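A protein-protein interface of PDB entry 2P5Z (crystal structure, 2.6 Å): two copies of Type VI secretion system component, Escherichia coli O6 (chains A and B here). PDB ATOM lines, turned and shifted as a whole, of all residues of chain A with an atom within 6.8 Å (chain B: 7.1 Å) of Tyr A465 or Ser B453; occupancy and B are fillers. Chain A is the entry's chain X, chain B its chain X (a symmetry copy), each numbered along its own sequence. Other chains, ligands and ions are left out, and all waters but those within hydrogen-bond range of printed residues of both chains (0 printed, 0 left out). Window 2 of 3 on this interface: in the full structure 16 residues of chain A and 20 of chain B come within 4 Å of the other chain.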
ATOM      1  N   THR A 386     -10.702  22.030  -2.498  1.00  0.00           N
ATOM      2  CA  THR A 386      -9.829  22.730  -3.401  1.00  0.00           C
ATOM      3  C   THR A 386      -9.634  24.184  -2.965  1.00  0.00           C
ATOM      4  O   THR A 386     -10.498  24.767  -2.304  1.00  0.00           O
ATOM      5  CB  THR A 386     -10.406  22.628  -4.822  1.00  0.00           C
ATOM      6  OG1 THR A 386      -9.336  22.660  -5.761  1.00  0.00           O
ATOM      7  CG2 THR A 386     -11.381  23.747  -5.113  1.00  0.00           C
ATOM      8  N   LEU A 427       2.329  30.985  -4.864  1.00  0.00           N
ATOM      9  CA  LEU A 427       2.533  29.553  -4.909  1.00  0.00           C
ATOM     10  C   LEU A 427       2.912  29.111  -6.316  1.00  0.00           C
ATOM     11  O   LEU A 427       2.242  29.480  -7.282  1.00  0.00           O
ATOM     12  CB  LEU A 427       1.222  28.890  -4.489  1.00  0.00           C
ATOM     13  CG  LEU A 427       1.108  27.493  -3.889  1.00  0.00           C
ATOM     14  CD1 LEU A 427       0.680  26.544  -4.942  1.00  0.00           C
ATOM     15  CD2 LEU A 427       2.378  27.017  -3.199  1.00  0.00           C
ATOM     16  N   VAL A 429       3.010  26.405  -9.047  1.00  0.00           N
ATOM     17  CA  VAL A 429       2.145  25.242  -9.199  1.00  0.00           C
ATOM     18  C   VAL A 429       1.959  24.733 -10.649  1.00  0.00           C
ATOM     19  O   VAL A 429       1.930  25.514 -11.598  1.00  0.00           O
ATOM     20  CB  VAL A 429       0.805  25.517  -8.450  1.00  0.00           C
ATOM     21  CG1 VAL A 429      -0.153  26.397  -9.248  1.00  0.00           C
ATOM     22  CG2 VAL A 429       0.159  24.256  -7.989  1.00  0.00           C
ATOM     23  N   ARG A 430       1.866  23.415 -10.809  1.00  0.00           N
ATOM     24  CA  ARG A 430       1.644  22.807 -12.122  1.00  0.00           C
ATOM     25  C   ARG A 430       0.179  22.478 -12.347  1.00  0.00           C
ATOM     26  O   ARG A 430      -0.437  21.802 -11.532  1.00  0.00           O
ATOM     27  CB  ARG A 430       2.483  21.540 -12.283  1.00  0.00           C
ATOM     28  CG  ARG A 430       3.954  21.821 -12.462  1.00  0.00           C
ATOM     29  CD  ARG A 430       4.723  20.618 -12.966  1.00  0.00           C
ATOM     30  NE  ARG A 430       6.159  20.889 -13.009  1.00  0.00           N
ATOM     31  CZ  ARG A 430       7.071  20.050 -13.494  1.00  0.00           C
ATOM     32  NH1 ARG A 430       6.708  18.873 -13.992  1.00  0.00           N
ATOM     33  NH2 ARG A 430       8.351  20.393 -13.484  1.00  0.00           N
ATOM     34  N   SER A 453      -8.392  26.221  -9.611  1.00  0.00           N
ATOM     35  CA  SER A 453      -8.616  25.443  -8.412  1.00  0.00           C
ATOM     36  C   SER A 453      -7.361  24.673  -8.078  1.00  0.00           C
ATOM     37  O   SER A 453      -6.808  23.979  -8.935  1.00  0.00           O
ATOM     38  CB  SER A 453      -9.780  24.490  -8.602  1.00  0.00           C
ATOM     39  OG  SER A 453     -10.990  25.173  -8.343  1.00  0.00           O
ATOM     40  N   ILE A 454      -6.904  24.813  -6.837  1.00  0.00           N
ATOM     41  CA  ILE A 454      -5.722  24.095  -6.383  1.00  0.00           C
ATOM     42  C   ILE A 454      -6.096  22.864  -5.547  1.00  0.00           C
ATOM     43  O   ILE A 454      -6.846  22.954  -4.566  1.00  0.00           O
ATOM     44  CB  ILE A 454      -4.778  25.013  -5.606  1.00  0.00           C
ATOM     45  CG1 ILE A 454      -4.544  26.299  -6.396  1.00  0.00           C
ATOM     46  CG2 ILE A 454      -3.460  24.307  -5.337  1.00  0.00           C
ATOM     47  CD1 ILE A 454      -3.708  26.087  -7.632  1.00  0.00           C
ATOM     48  N   ALA A 455      -5.587  21.716  -5.971  1.00  0.00           N
ATOM     49  CA  ALA A 455      -5.834  20.461  -5.299  1.00  0.00           C
ATOM     50  C   ALA A 455      -4.516  19.919  -4.769  1.00  0.00           C
ATOM     51  O   ALA A 455      -3.452  20.389  -5.135  1.00  0.00           O
ATOM     52  CB  ALA A 455      -6.477  19.455  -6.249  1.00  0.00           C
ATOM     53  N   PHE A 456      -4.597  18.914  -3.901  1.00  0.00           N
ATOM     54  CA  PHE A 456      -3.440  18.474  -3.142  1.00  0.00           C
ATOM     55  C   PHE A 456      -3.364  16.981  -3.155  1.00  0.00           C
ATOM     56  O   PHE A 456      -4.310  16.296  -2.760  1.00  0.00           O
ATOM     57  CB  PHE A 456      -3.531  18.991  -1.709  1.00  0.00           C
ATOM     58  CG  PHE A 456      -3.500  20.490  -1.609  1.00  0.00           C
ATOM     59  CD1 PHE A 456      -2.300  21.156  -1.566  1.00  0.00           C
ATOM     60  CD2 PHE A 456      -4.672  21.224  -1.604  1.00  0.00           C
ATOM     61  CE1 PHE A 456      -2.263  22.525  -1.480  1.00  0.00           C
ATOM     62  CE2 PHE A 456      -4.636  22.600  -1.529  1.00  0.00           C
ATOM     63  CZ  PHE A 456      -3.422  23.251  -1.466  1.00  0.00           C
ATOM     64  N   GLU A 457      -2.236  16.483  -3.627  1.00  0.00           N
ATOM     65  CA  GLU A 457      -2.063  15.066  -3.827  1.00  0.00           C
ATOM     66  C   GLU A 457      -1.998  14.366  -2.463  1.00  0.00           C
ATOM     67  O   GLU A 457      -1.204  14.747  -1.604  1.00  0.00           O
ATOM     68  CB  GLU A 457      -0.801  14.844  -4.643  1.00  0.00           C
ATOM     69  CG  GLU A 457      -0.623  13.454  -5.123  1.00  0.00           C
ATOM     70  CD  GLU A 457       0.516  13.348  -6.094  1.00  0.00           C
ATOM     71  OE1 GLU A 457       1.683  13.550  -5.683  1.00  0.00           O
ATOM     72  OE2 GLU A 457       0.240  13.063  -7.275  1.00  0.00           O
ATOM     73  N   GLU A 458      -2.853  13.356  -2.292  1.00  0.00           N
ATOM     74  CA  GLU A 458      -3.206  12.715  -0.997  1.00  0.00           C
ATOM     75  C   GLU A 458      -3.408  13.626   0.229  1.00  0.00           C
ATOM     76  O   GLU A 458      -3.040  13.265   1.331  1.00  0.00           O
ATOM     77  CB  GLU A 458      -2.359  11.464  -0.677  1.00  0.00           C
ATOM     78  CG  GLU A 458      -0.840  11.596  -0.781  1.00  0.00           C
ATOM     79  CD  GLU A 458      -0.158  10.261  -1.026  1.00  0.00           C
ATOM     80  OE1 GLU A 458      -0.433   9.305  -0.262  1.00  0.00           O
ATOM     81  OE2 GLU A 458       0.651  10.168  -1.981  1.00  0.00           O
ATOM     82  N   ARG A 463       1.984  19.258  -1.722  1.00  0.00           N
ATOM     83  CA  ARG A 463       1.895  18.694  -3.059  1.00  0.00           C
ATOM     84  C   ARG A 463       0.770  19.319  -3.873  1.00  0.00           C
ATOM     85  O   ARG A 463      -0.157  18.615  -4.276  1.00  0.00           O
ATOM     86  CB  ARG A 463       1.651  17.195  -2.985  1.00  0.00           C
ATOM     87  CG  ARG A 463       2.813  16.346  -2.548  1.00  0.00           C
ATOM     88  CD  ARG A 463       2.315  14.928  -2.566  1.00  0.00           C
ATOM     89  NE  ARG A 463       3.355  13.923  -2.426  1.00  0.00           N
ATOM     90  CZ  ARG A 463       3.139  12.617  -2.575  1.00  0.00           C
ATOM     91  NH1 ARG A 463       1.927  12.170  -2.880  1.00  0.00           N
ATOM     92  NH2 ARG A 463       4.137  11.757  -2.421  1.00  0.00           N
ATOM     93  N   PRO A 464       0.844  20.633  -4.142  1.00  0.00           N
ATOM     94  CA  PRO A 464      -0.298  21.212  -4.817  1.00  0.00           C
ATOM     95  C   PRO A 464      -0.226  21.105  -6.342  1.00  0.00           C
ATOM     96  O   PRO A 464       0.865  21.055  -6.928  1.00  0.00           O
ATOM     97  CB  PRO A 464      -0.230  22.675  -4.397  1.00  0.00           C
ATOM     98  CG  PRO A 464       1.207  22.928  -4.170  1.00  0.00           C
ATOM     99  CD  PRO A 464       1.890  21.639  -3.894  1.00  0.00           C
ATOM    100  N   TYR A 465      -1.391  21.081  -6.976  1.00  0.00           N
ATOM    101  CA  TYR A 465      -1.461  21.109  -8.419  1.00  0.00           C
ATOM    102  C   TYR A 465      -2.741  21.803  -8.847  1.00  0.00           C
ATOM    103  O   TYR A 465      -3.653  21.981  -8.034  1.00  0.00           O
ATOM    104  CB  TYR A 465      -1.326  19.706  -9.031  1.00  0.00           C
ATOM    105  CG  TYR A 465      -2.475  18.780  -8.750  1.00  0.00           C
ATOM    106  CD1 TYR A 465      -2.448  17.918  -7.650  1.00  0.00           C
ATOM    107  CD2 TYR A 465      -3.593  18.747  -9.590  1.00  0.00           C
ATOM    108  CE1 TYR A 465      -3.514  17.065  -7.389  1.00  0.00           C
ATOM    109  CE2 TYR A 465      -4.659  17.902  -9.336  1.00  0.00           C
ATOM    110  CZ  TYR A 465      -4.612  17.062  -8.236  1.00  0.00           C
ATOM    111  OH  TYR A 465      -5.679  16.235  -7.991  1.00  0.00           O
ATOM    112  N   ILE A 466      -2.808  22.188 -10.124  1.00  0.00           N
ATOM    113  CA  ILE A 466      -4.017  22.802 -10.699  1.00  0.00           C
ATOM    114  C   ILE A 466      -5.011  21.730 -11.138  1.00  0.00           C
ATOM    115  O   ILE A 466      -4.650  20.822 -11.879  1.00  0.00           O
ATOM    116  CB  ILE A 466      -3.665  23.718 -11.891  1.00  0.00           C
ATOM    117  CG1 ILE A 466      -2.544  24.673 -11.484  1.00  0.00           C
ATOM    118  CG2 ILE A 466      -4.873  24.500 -12.355  1.00  0.00           C
ATOM    119  CD1 ILE A 466      -2.409  25.888 -12.352  1.00  0.00           C
ATOM    120  N   ALA A 467      -6.253  21.830 -10.675  1.00  0.00           N
ATOM    121  CA  ALA A 467      -7.231  20.776 -10.944  1.00  0.00           C
ATOM    122  C   ALA A 467      -7.984  20.763 -12.304  1.00  0.00           C
ATOM    123  O   ALA A 467      -7.969  19.711 -12.933  1.00  0.00           O
ATOM    124  CB  ALA A 467      -8.173  20.519  -9.730  1.00  0.00           C
ATOM    125  N   GLY A 468      -8.665  21.825 -12.777  1.00  0.00           N
ATOM    126  CA  GLY A 468      -9.079  23.008 -12.044  1.00  0.00           C
ATOM    127  C   GLY A 468      -8.964  24.378 -12.698  1.00  0.00           C
ATOM    128  O   GLY A 468      -8.090  25.147 -12.317  1.00  0.00           O
ATOM    129  N   GLY B 385      -8.219  14.482  -1.062  1.00  0.00           N
ATOM    130  CA  GLY B 385      -7.170  14.570  -2.066  1.00  0.00           C
ATOM    131  C   GLY B 385      -7.138  13.386  -3.019  1.00  0.00           C
ATOM    132  O   GLY B 385      -8.047  12.547  -3.061  1.00  0.00           O
ATOM    133  N   THR B 386      -6.049  13.297  -3.758  1.00  0.00           N
ATOM    134  CA  THR B 386      -5.992  12.422  -4.897  1.00  0.00           C
ATOM    135  C   THR B 386      -4.790  11.479  -4.809  1.00  0.00           C
ATOM    136  O   THR B 386      -3.780  11.798  -4.176  1.00  0.00           O
ATOM    137  CB  THR B 386      -5.958  13.278  -6.174  1.00  0.00           C
ATOM    138  OG1 THR B 386      -6.577  12.555  -7.233  1.00  0.00           O
ATOM    139  CG2 THR B 386      -4.545  13.653  -6.561  1.00  0.00           C
ATOM    140  N   LEU B 387      -4.895  10.298  -5.405  1.00  0.00           N
ATOM    141  CA  LEU B 387      -3.732   9.399  -5.435  1.00  0.00           C
ATOM    142  C   LEU B 387      -3.122   9.338  -6.831  1.00  0.00           C
ATOM    143  O   LEU B 387      -3.843   9.170  -7.819  1.00  0.00           O
ATOM    144  CB  LEU B 387      -4.091   7.986  -4.971  1.00  0.00           C
ATOM    145  CG  LEU B 387      -4.536   7.817  -3.528  1.00  0.00           C
ATOM    146  CD1 LEU B 387      -4.823   6.352  -3.276  1.00  0.00           C
ATOM    147  CD2 LEU B 387      -3.448   8.350  -2.604  1.00  0.00           C
ATOM    148  N   PRO B 388      -1.797   9.483  -6.917  1.00  0.00           N
ATOM    149  CA  PRO B 388      -1.142   9.324  -8.208  1.00  0.00           C
ATOM    150  C   PRO B 388      -1.122   7.856  -8.624  1.00  0.00           C
ATOM    151  O   PRO B 388      -0.977   6.968  -7.778  1.00  0.00           O
ATOM    152  CB  PRO B 388       0.280   9.822  -7.950  1.00  0.00           C
ATOM    153  CG  PRO B 388       0.505   9.609  -6.487  1.00  0.00           C
ATOM    154  CD  PRO B 388      -0.845   9.786  -5.831  1.00  0.00           C
ATOM    155  N   ALA B 389      -1.308   7.600  -9.914  1.00  0.00           N
ATOM    156  CA  ALA B 389      -1.157   6.251 -10.419  1.00  0.00           C
ATOM    157  C   ALA B 389      -0.508   6.267 -11.793  1.00  0.00           C
ATOM    158  O   ALA B 389      -0.473   7.302 -12.455  1.00  0.00           O
ATOM    159  CB  ALA B 389      -2.480   5.570 -10.470  1.00  0.00           C
ATOM    160  N   VAL B 429      -9.923   0.965 -12.867  1.00  0.00           N
ATOM    161  CA  VAL B 429     -10.506   2.284 -12.652  1.00  0.00           C
ATOM    162  C   VAL B 429     -11.021   3.001 -13.923  1.00  0.00           C
ATOM    163  O   VAL B 429     -10.449   2.871 -15.003  1.00  0.00           O
ATOM    164  CB  VAL B 429      -9.511   3.136 -11.804  1.00  0.00           C
ATOM    165  CG1 VAL B 429      -8.372   3.720 -12.634  1.00  0.00           C
ATOM    166  CG2 VAL B 429     -10.217   4.176 -11.005  1.00  0.00           C
ATOM    167  N   GLU B 451       0.752   9.170 -16.172  1.00  0.00           N
ATOM    168  CA  GLU B 451       0.446   9.354 -14.760  1.00  0.00           C
ATOM    169  C   GLU B 451      -0.899  10.032 -14.564  1.00  0.00           C
ATOM    170  O   GLU B 451      -1.150  11.114 -15.093  1.00  0.00           O
ATOM    171  CB  GLU B 451       1.561  10.114 -14.037  1.00  0.00           C
ATOM    172  CG  GLU B 451       2.817   9.268 -13.809  1.00  0.00           C
ATOM    173  CD  GLU B 451       3.993  10.061 -13.228  1.00  0.00           C
ATOM    174  OE1 GLU B 451       3.768  11.158 -12.658  1.00  0.00           O
ATOM    175  OE2 GLU B 451       5.149   9.585 -13.341  1.00  0.00           O
ATOM    176  N   VAL B 452      -1.767   9.376 -13.809  1.00  0.00           N
ATOM    177  CA  VAL B 452      -3.097   9.911 -13.564  1.00  0.00           C
ATOM    178  C   VAL B 452      -3.348  10.232 -12.093  1.00  0.00           C
ATOM    179  O   VAL B 452      -2.566   9.863 -11.216  1.00  0.00           O
ATOM    180  CB  VAL B 452      -4.173   8.947 -14.034  1.00  0.00           C
ATOM    181  CG1 VAL B 452      -4.182   8.889 -15.551  1.00  0.00           C
ATOM    182  CG2 VAL B 452      -3.943   7.580 -13.422  1.00  0.00           C
ATOM    183  N   SER B 453      -4.446  10.932 -11.840  1.00  0.00           N
ATOM    184  CA  SER B 453      -4.861  11.221 -10.485  1.00  0.00           C
ATOM    185  C   SER B 453      -6.109  10.435 -10.168  1.00  0.00           C
ATOM    186  O   SER B 453      -7.083  10.476 -10.926  1.00  0.00           O
ATOM    187  CB  SER B 453      -5.120  12.706 -10.311  1.00  0.00           C
ATOM    188  OG  SER B 453      -3.898  13.364 -10.043  1.00  0.00           O
ATOM    189  N   ILE B 454      -6.072   9.704  -9.057  1.00  0.00           N
ATOM    190  CA  ILE B 454      -7.225   8.929  -8.625  1.00  0.00           C
ATOM    191  C   ILE B 454      -7.996   9.640  -7.505  1.00  0.00           C
ATOM    192  O   ILE B 454      -7.428  10.024  -6.474  1.00  0.00           O
ATOM    193  CB  ILE B 454      -6.818   7.520  -8.194  1.00  0.00           C
ATOM    194  CG1 ILE B 454      -5.925   6.891  -9.262  1.00  0.00           C
ATOM    195  CG2 ILE B 454      -8.051   6.663  -7.962  1.00  0.00           C
ATOM    196  CD1 ILE B 454      -6.670   6.549 -10.526  1.00  0.00           C
ATOM    197  N   ALA B 455      -9.285   9.836  -7.741  1.00  0.00           N
ATOM    198  CA  ALA B 455     -10.160  10.486  -6.792  1.00  0.00           C
ATOM    199  C   ALA B 455     -11.221   9.495  -6.342  1.00  0.00           C
ATOM    200  O   ALA B 455     -11.393   8.445  -6.939  1.00  0.00           O
ATOM    201  CB  ALA B 455     -10.813  11.717  -7.413  1.00  0.00           C
ATOM    202  N   TYR B 465     -12.046   6.765  -9.145  1.00  0.00           N
ATOM    203  CA  TYR B 465     -12.158   7.131 -10.538  1.00  0.00           C
ATOM    204  C   TYR B 465     -10.972   7.997 -10.926  1.00  0.00           C
ATOM    205  O   TYR B 465     -10.268   8.513 -10.055  1.00  0.00           O
ATOM    206  CB  TYR B 465     -13.501   7.808 -10.852  1.00  0.00           C
ATOM    207  CG  TYR B 465     -13.687   9.162 -10.229  1.00  0.00           C
ATOM    208  CD1 TYR B 465     -14.312   9.299  -8.987  1.00  0.00           C
ATOM    209  CD2 TYR B 465     -13.256  10.320 -10.885  1.00  0.00           C
ATOM    210  CE1 TYR B 465     -14.479  10.552  -8.410  1.00  0.00           C
ATOM    211  CE2 TYR B 465     -13.418  11.571 -10.318  1.00  0.00           C
ATOM    212  CZ  TYR B 465     -14.032  11.682  -9.082  1.00  0.00           C
ATOM    213  OH  TYR B 465     -14.180  12.927  -8.526  1.00  0.00           O
ATOM    214  N   ILE B 466     -10.760   8.155 -12.235  1.00  0.00           N
ATOM    215  CA  ILE B 466      -9.695   9.029 -12.760  1.00  0.00           C
ATOM    216  C   ILE B 466     -10.170  10.479 -12.824  1.00  0.00           C
ATOM    217  O   ILE B 466     -11.217  10.759 -13.398  1.00  0.00           O
ATOM    218  CB  ILE B 466      -9.227   8.563 -14.155  1.00  0.00           C
ATOM    219  CG1 ILE B 466      -8.920   7.067 -14.113  1.00  0.00           C
ATOM    220  CG2 ILE B 466      -8.006   9.333 -14.607  1.00  0.00           C
ATOM    221  CD1 ILE B 466      -8.047   6.574 -15.228  1.00  0.00           C
ATOM    222  N   ALA B 467      -9.409  11.393 -12.230  1.00  0.00           N
ATOM    223  CA  ALA B 467      -9.856  12.782 -12.136  1.00  0.00           C
ATOM    224  C   ALA B 467      -9.651  13.733 -13.349  1.00  0.00           C
ATOM    225  O   ALA B 467     -10.636  14.351 -13.738  1.00  0.00           O
ATOM    226  CB  ALA B 467      -9.463  13.439 -10.780  1.00  0.00           C
ATOM    227  N   GLY B 468      -8.456  13.923 -13.939  1.00  0.00           N
ATOM    228  CA  GLY B 468      -7.146  13.561 -13.424  1.00  0.00           C
ATOM    229  C   GLY B 468      -6.106  12.966 -14.362  1.00  0.00           C
ATOM    230  O   GLY B 468      -5.838  11.774 -14.274  1.00  0.00           O
ATOM    231  N   VAL B 469      -5.490  13.772 -15.237  1.00  0.00           N
ATOM    232  CA  VAL B 469      -4.247  13.343 -15.942  1.00  0.00           C
ATOM    233  C   VAL B 469      -3.069  14.286 -15.636  1.00  0.00           C
ATOM    234  O   VAL B 469      -3.177  15.501 -15.810  1.00  0.00           O
ATOM    235  CB  VAL B 469      -4.417  13.206 -17.492  1.00  0.00           C
ATOM    236  CG1 VAL B 469      -3.166  12.577 -18.129  1.00  0.00           C
ATOM    237  CG2 VAL B 469      -5.651  12.389 -17.854  1.00  0.00           C
ATOM    238  N   LYS B 470      -1.946  13.742 -15.182  1.00  0.00           N
ATOM    239  CA  LYS B 470      -0.818  14.594 -14.797  1.00  0.00           C
ATOM    240  C   LYS B 470       0.139  14.887 -15.951  1.00  0.00           C
ATOM    241  O   LYS B 470       1.231  14.322 -16.022  1.00  0.00           O
ATOM    242  CB  LYS B 470      -0.059  13.995 -13.611  1.00  0.00           C
ATOM    243  CG  LYS B 470      -0.926  13.826 -12.371  1.00  0.00           C
ATOM    244  CD  LYS B 470      -0.124  13.982 -11.082  1.00  0.00           C
ATOM    245  CE  LYS B 470       0.752  12.775 -10.814  1.00  0.00           C
ATOM    246  NZ  LYS B 470       1.662  13.037  -9.659  1.00  0.00           N
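The side-chain amino group (NZ) of Lys B470 is in salt-bridge range of the side-chain carboxylate (OE2) of Glu A457, 2.8 Å away. N of Glu A458 is in hydrogen-bond range of O of Thr B386, 2.6 Å away.
The backbone NH (N) of Ala A455 is in hydrogen-bond range of the backbone carbonyl oxygen (O) of Tyr A465. The guanidinium group of Arg A463 lies within salt-bridge range of the side-chain carboxylate of Glu A457 (3.1 Å). The side-chain carboxylate of Glu A458 lies within salt-bridge range of the guanidinium group of Arg A463, at 2.5 Å. OG1 of Thr B386 is in hydrogen-bond range of O of Ile B454. The backbone NH (N) of Ala B467 sits at hydrogen-bond distance from the backbone carbonyl oxygen (O) of Ser B453 (2.8 Å). The backbone NH (N) of Ser B453 is in hydrogen-bond range of the backbone carbonyl oxygen (O) of Gly B468 (2.9 Å).
Gly B385 touches Phe A456 (CA to O, 3.4 Å). Phe A456 touches Thr B386. Glu A457 touches Thr B386. Glu A457 touches Pro B388. Glu A458 touches Leu B387 (CB to CD2, 3.8 Å). Thr B386 touches Tyr A465. OH of Tyr A465 touches OG of Ser B453, 3.95 Å away.
Tyr A465 touches two residues of chain B. Of chain A, only Tyr A465 comes within 4 Å of Ser B453. Printed residues of chain A within 4 Å of Lys B470: Glu A457 (2.8 Å). Printed residues of chain B within 4 Å of Glu A457: Thr B386 (3.6 Å), Pro B388 (3.3 Å) and Lys B470 (2.8 Å). Glu B451 touches none of the printed residues of chain A. The nearest residue of chain B that does not touch Tyr A465 is Ala B467 (5.5 Å). The nearest residue of chain A that does not touch Ser B453 is Glu A457 (5.0 Å).
Of the 16 printed residues of chain A, 4 touch a printed residue of chain B. Printed residues of chain A that touch a printed residue of chain B: Phe A456, Glu A457, Glu A458 and Tyr A465. Hydrophobic or aromatic side chains of chain A that line the printed part of chain B: Tyr A465. Hydrophobic or aromatic side chains of chain B that line the printed part of chain A: Leu B387 and Pro B388. Along chain B the printed residues that touch a printed residue of chain A span positions 385 to 470. Among the printed residues, 9 pairs touch across the chains. Among the printed residues, Asp or Glu carboxylates within 4 Å of a Lys or Arg side-chain nitrogen of the other chain: Glu A457 with Lys B470.
Tyr A465 touches Thr B386, but with the chains exchanged Thr A386 does not touch Tyr B465 (11.0 Å). Tyr A465 touches Ser B453, but with the chains exchanged Ser A453 does not touch Tyr B465 (12.4 Å). Positions printed for both chains: 386, 429, 453, 454, 455, 465, 466, 467 and 468.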
